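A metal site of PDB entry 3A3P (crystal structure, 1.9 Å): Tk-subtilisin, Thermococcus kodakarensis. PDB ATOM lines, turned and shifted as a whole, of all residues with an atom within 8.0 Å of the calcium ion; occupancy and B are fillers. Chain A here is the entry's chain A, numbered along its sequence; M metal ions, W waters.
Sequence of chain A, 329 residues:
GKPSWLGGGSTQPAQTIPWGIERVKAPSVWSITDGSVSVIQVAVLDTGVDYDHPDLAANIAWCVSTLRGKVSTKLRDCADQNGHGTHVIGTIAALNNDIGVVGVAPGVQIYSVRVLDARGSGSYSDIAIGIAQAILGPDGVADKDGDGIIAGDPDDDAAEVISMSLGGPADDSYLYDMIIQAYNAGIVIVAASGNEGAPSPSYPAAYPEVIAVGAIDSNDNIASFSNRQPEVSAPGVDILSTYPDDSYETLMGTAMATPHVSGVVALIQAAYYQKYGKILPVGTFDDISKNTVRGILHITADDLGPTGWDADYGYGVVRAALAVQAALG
N of Tyr 313 is in hydrogen-bond range of OD2 of Asp 310. OD2 of Asp 310 lies within hydrogen-bond range of N of Asp 312, at 3.0 Å.
The nearest printed residue that does not touch the calcium ion is Gly 305 (4.01 Å).
The calcium ion is bound by OD1 of Asp 303 (2.3 Å), OD1 of Asp 310 (2.3 Å), O of Pro 306 (2.3 Å), O of Leu 304 (2.3 Å), O of Gly 308 (2.4 Å) and water W1 (2.4 Å). The calcium ion has six donor atoms within binding distance.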
ATOM      1  N   ASP A 302     -26.752 -11.420  14.862  1.00  0.00           N
ATOM      2  CA  ASP A 302     -27.287 -12.126  16.035  1.00  0.00           C
ATOM      3  C   ASP A 302     -26.127 -12.480  16.981  1.00  0.00           C
ATOM      4  O   ASP A 302     -25.304 -13.357  16.677  1.00  0.00           O
ATOM      5  CB  ASP A 302     -28.082 -13.370  15.621  1.00  0.00           C
ATOM      6  CG  ASP A 302     -28.912 -13.924  16.748  1.00  0.00           C
ATOM      7  OD1 ASP A 302     -28.821 -13.398  17.872  1.00  0.00           O
ATOM      8  OD2 ASP A 302     -29.629 -14.905  16.526  1.00  0.00           O
ATOM      9  N   ASP A 303     -26.062 -11.794  18.114  1.00  0.00           N
ATOM     10  CA  ASP A 303     -24.969 -11.960  19.074  1.00  0.00           C
ATOM     11  C   ASP A 303     -25.077 -13.248  19.896  1.00  0.00           C
ATOM     12  O   ASP A 303     -25.671 -13.252  20.993  1.00  0.00           O
ATOM     13  CB  ASP A 303     -24.892 -10.733  20.001  1.00  0.00           C
ATOM     14  CG  ASP A 303     -23.736 -10.807  21.012  1.00  0.00           C
ATOM     15  OD1 ASP A 303     -22.825 -11.696  20.911  1.00  0.00           O
ATOM     16  OD2 ASP A 303     -23.742  -9.946  21.923  1.00  0.00           O
ATOM     17  N   LEU A 304     -24.479 -14.316  19.392  1.00  0.00           N
ATOM     18  CA  LEU A 304     -24.442 -15.608  20.045  1.00  0.00           C
ATOM     19  C   LEU A 304     -23.247 -15.718  20.998  1.00  0.00           C
ATOM     20  O   LEU A 304     -22.370 -14.873  20.976  1.00  0.00           O
ATOM     21  CB  LEU A 304     -24.329 -16.686  18.991  1.00  0.00           C
ATOM     22  CG  LEU A 304     -25.521 -16.776  18.007  1.00  0.00           C
ATOM     23  CD1 LEU A 304     -25.374 -17.991  17.115  1.00  0.00           C
ATOM     24  CD2 LEU A 304     -26.878 -16.809  18.728  1.00  0.00           C
ATOM     25  N   GLY A 305     -23.173 -16.790  21.784  1.00  0.00           N
ATOM     26  CA  GLY A 305     -22.035 -16.999  22.675  1.00  0.00           C
ATOM     27  C   GLY A 305     -22.015 -15.902  23.739  1.00  0.00           C
ATOM     28  O   GLY A 305     -23.071 -15.337  24.048  1.00  0.00           O
ATOM     29  N   PRO A 306     -20.809 -15.590  24.297  1.00  0.00           N
ATOM     30  CA  PRO A 306     -20.698 -14.542  25.312  1.00  0.00           C
ATOM     31  C   PRO A 306     -21.125 -13.203  24.731  1.00  0.00           C
ATOM     32  O   PRO A 306     -21.061 -13.042  23.514  1.00  0.00           O
ATOM     33  CB  PRO A 306     -19.192 -14.500  25.629  1.00  0.00           C
ATOM     34  CG  PRO A 306     -18.644 -15.830  25.142  1.00  0.00           C
ATOM     35  CD  PRO A 306     -19.516 -16.215  23.968  1.00  0.00           C
ATOM     36  N   THR A 307     -21.511 -12.246  25.572  1.00  0.00           N
ATOM     37  CA  THR A 307     -21.957 -10.958  25.078  1.00  0.00           C
ATOM     38  C   THR A 307     -20.850 -10.291  24.258  1.00  0.00           C
ATOM     39  O   THR A 307     -19.677 -10.396  24.594  1.00  0.00           O
ATOM     40  CB  THR A 307     -22.434 -10.060  26.246  1.00  0.00           C
ATOM     41  OG1 THR A 307     -23.664 -10.597  26.733  1.00  0.00           O
ATOM     42  CG2 THR A 307     -22.677  -8.601  25.819  1.00  0.00           C
ATOM     43  N   GLY A 308     -21.228  -9.654  23.155  1.00  0.00           N
ATOM     44  CA  GLY A 308     -20.303  -8.888  22.373  1.00  0.00           C
ATOM     45  C   GLY A 308     -19.514  -9.752  21.418  1.00  0.00           C
ATOM     46  O   GLY A 308     -19.771 -10.967  21.305  1.00  0.00           O
ATOM     47  N   TRP A 309     -18.567  -9.135  20.704  1.00  0.00           N
ATOM     48  CA  TRP A 309     -17.651  -9.881  19.845  1.00  0.00           C
ATOM     49  C   TRP A 309     -16.971 -10.997  20.637  1.00  0.00           C
ATOM     50  O   TRP A 309     -16.530 -10.781  21.773  1.00  0.00           O
ATOM     51  CB  TRP A 309     -16.608  -8.945  19.222  1.00  0.00           C
ATOM     52  CG  TRP A 309     -15.707  -9.646  18.221  1.00  0.00           C
ATOM     53  CD1 TRP A 309     -15.886  -9.710  16.861  1.00  0.00           C
ATOM     54  CD2 TRP A 309     -14.524 -10.387  18.506  1.00  0.00           C
ATOM     55  NE1 TRP A 309     -14.870 -10.426  16.285  1.00  0.00           N
ATOM     56  CE2 TRP A 309     -14.024 -10.867  17.263  1.00  0.00           C
ATOM     57  CE3 TRP A 309     -13.811 -10.695  19.697  1.00  0.00           C
ATOM     58  CZ2 TRP A 309     -12.873 -11.653  17.175  1.00  0.00           C
ATOM     59  CZ3 TRP A 309     -12.667 -11.469  19.606  1.00  0.00           C
ATOM     60  CH2 TRP A 309     -12.191 -11.948  18.349  1.00  0.00           C
ATOM     61  N   ASP A 310     -16.889 -12.188  20.060  1.00  0.00           N
ATOM     62  CA  ASP A 310     -16.159 -13.263  20.723  1.00  0.00           C
ATOM     63  C   ASP A 310     -15.354 -14.069  19.712  1.00  0.00           C
ATOM     64  O   ASP A 310     -15.619 -13.974  18.512  1.00  0.00           O
ATOM     65  CB  ASP A 310     -17.111 -14.129  21.546  1.00  0.00           C
ATOM     66  CG  ASP A 310     -18.110 -14.866  20.690  1.00  0.00           C
ATOM     67  OD1 ASP A 310     -19.257 -14.394  20.612  1.00  0.00           O
ATOM     68  OD2 ASP A 310     -17.758 -15.905  20.106  1.00  0.00           O
ATOM     69  N   ALA A 311     -14.379 -14.850  20.176  1.00  0.00           N
ATOM     70  CA  ALA A 311     -13.451 -15.530  19.271  1.00  0.00           C
ATOM     71  C   ALA A 311     -14.110 -16.618  18.414  1.00  0.00           C
ATOM     72  O   ALA A 311     -13.560 -17.028  17.387  1.00  0.00           O
ATOM     73  CB  ALA A 311     -12.287 -16.095  20.042  1.00  0.00           C
ATOM     74  N   ASP A 312     -15.284 -17.080  18.835  1.00  0.00           N
ATOM     75  CA  ASP A 312     -16.005 -18.106  18.090  1.00  0.00           C
ATOM     76  C   ASP A 312     -16.852 -17.529  16.950  1.00  0.00           C
ATOM     77  O   ASP A 312     -16.611 -17.869  15.768  1.00  0.00           O
ATOM     78  CB  ASP A 312     -16.897 -18.951  19.009  1.00  0.00           C
ATOM     79  CG  ASP A 312     -16.101 -19.895  19.878  1.00  0.00           C
ATOM     80  OD1 ASP A 312     -15.018 -20.330  19.455  1.00  0.00           O
ATOM     81  OD2 ASP A 312     -16.587 -20.223  20.982  1.00  0.00           O
ATOM     82  N   TYR A 313     -17.786 -16.639  17.290  1.00  0.00           N
ATOM     83  CA  TYR A 313     -18.791 -16.164  16.336  1.00  0.00           C
ATOM     84  C   TYR A 313     -18.473 -14.820  15.721  1.00  0.00           C
ATOM     85  O   TYR A 313     -19.239 -14.330  14.877  1.00  0.00           O
ATOM     86  CB  TYR A 313     -20.138 -16.016  17.020  1.00  0.00           C
ATOM     87  CG  TYR A 313     -20.712 -17.274  17.604  1.00  0.00           C
ATOM     88  CD1 TYR A 313     -20.564 -17.569  18.971  1.00  0.00           C
ATOM     89  CD2 TYR A 313     -21.421 -18.180  16.802  1.00  0.00           C
ATOM     90  CE1 TYR A 313     -21.118 -18.741  19.509  1.00  0.00           C
ATOM     91  CE2 TYR A 313     -21.963 -19.318  17.321  1.00  0.00           C
ATOM     92  CZ  TYR A 313     -21.810 -19.596  18.678  1.00  0.00           C
ATOM     93  OH  TYR A 313     -22.376 -20.758  19.182  1.00  0.00           O
ATOM     94  N   GLY A 314     -17.403 -14.181  16.176  1.00  0.00           N
ATOM     95  CA  GLY A 314     -17.186 -12.786  15.798  1.00  0.00           C
ATOM     96  C   GLY A 314     -18.263 -11.923  16.402  1.00  0.00           C
ATOM     97  O   GLY A 314     -18.600 -12.100  17.568  1.00  0.00           O
ATOM     98  N   TYR A 315     -18.815 -10.993  15.619  1.00  0.00           N
ATOM     99  CA  TYR A 315     -19.889 -10.180  16.117  1.00  0.00           C
ATOM    100  C   TYR A 315     -21.179 -10.962  16.224  1.00  0.00           C
ATOM    101  O   TYR A 315     -22.060 -10.580  16.974  1.00  0.00           O
ATOM    102  CB  TYR A 315     -20.144  -8.945  15.272  1.00  0.00           C
ATOM    103  CG  TYR A 315     -19.135  -7.847  15.458  1.00  0.00           C
ATOM    104  CD1 TYR A 315     -18.105  -7.703  14.560  1.00  0.00           C
ATOM    105  CD2 TYR A 315     -19.200  -6.975  16.560  1.00  0.00           C
ATOM    106  CE1 TYR A 315     -17.170  -6.672  14.689  1.00  0.00           C
ATOM    107  CE2 TYR A 315     -18.253  -5.949  16.709  1.00  0.00           C
ATOM    108  CZ  TYR A 315     -17.246  -5.811  15.765  1.00  0.00           C
ATOM    109  OH  TYR A 315     -16.283  -4.829  15.869  1.00  0.00           O
ATOM    110  N   GLY A 316     -21.310 -12.026  15.443  1.00  0.00           N
ATOM    111  CA  GLY A 316     -22.485 -12.897  15.487  1.00  0.00           C
ATOM    112  C   GLY A 316     -22.900 -13.346  14.107  1.00  0.00           C
ATOM    113  O   GLY A 316     -22.158 -13.152  13.159  1.00  0.00           O
ATOM    114  N   VAL A 317     -24.103 -13.905  14.003  1.00  0.00           N
ATOM    115  CA  VAL A 317     -24.637 -14.429  12.714  1.00  0.00           C
ATOM    116  C   VAL A 317     -25.295 -13.322  11.941  1.00  0.00           C
ATOM    117  O   VAL A 317     -26.214 -12.683  12.443  1.00  0.00           O
ATOM    118  CB  VAL A 317     -25.666 -15.553  12.974  1.00  0.00           C
ATOM    119  CG1 VAL A 317     -26.193 -16.166  11.639  1.00  0.00           C
ATOM    120  CG2 VAL A 317     -25.022 -16.619  13.873  1.00  0.00           C
HETATM  121 CA    CA M   1     -20.987 -12.995  21.176  1.00  0.00          CA
HETATM  122  O   HOH W   1     -21.037 -12.787  18.792  1.00  0.00           O
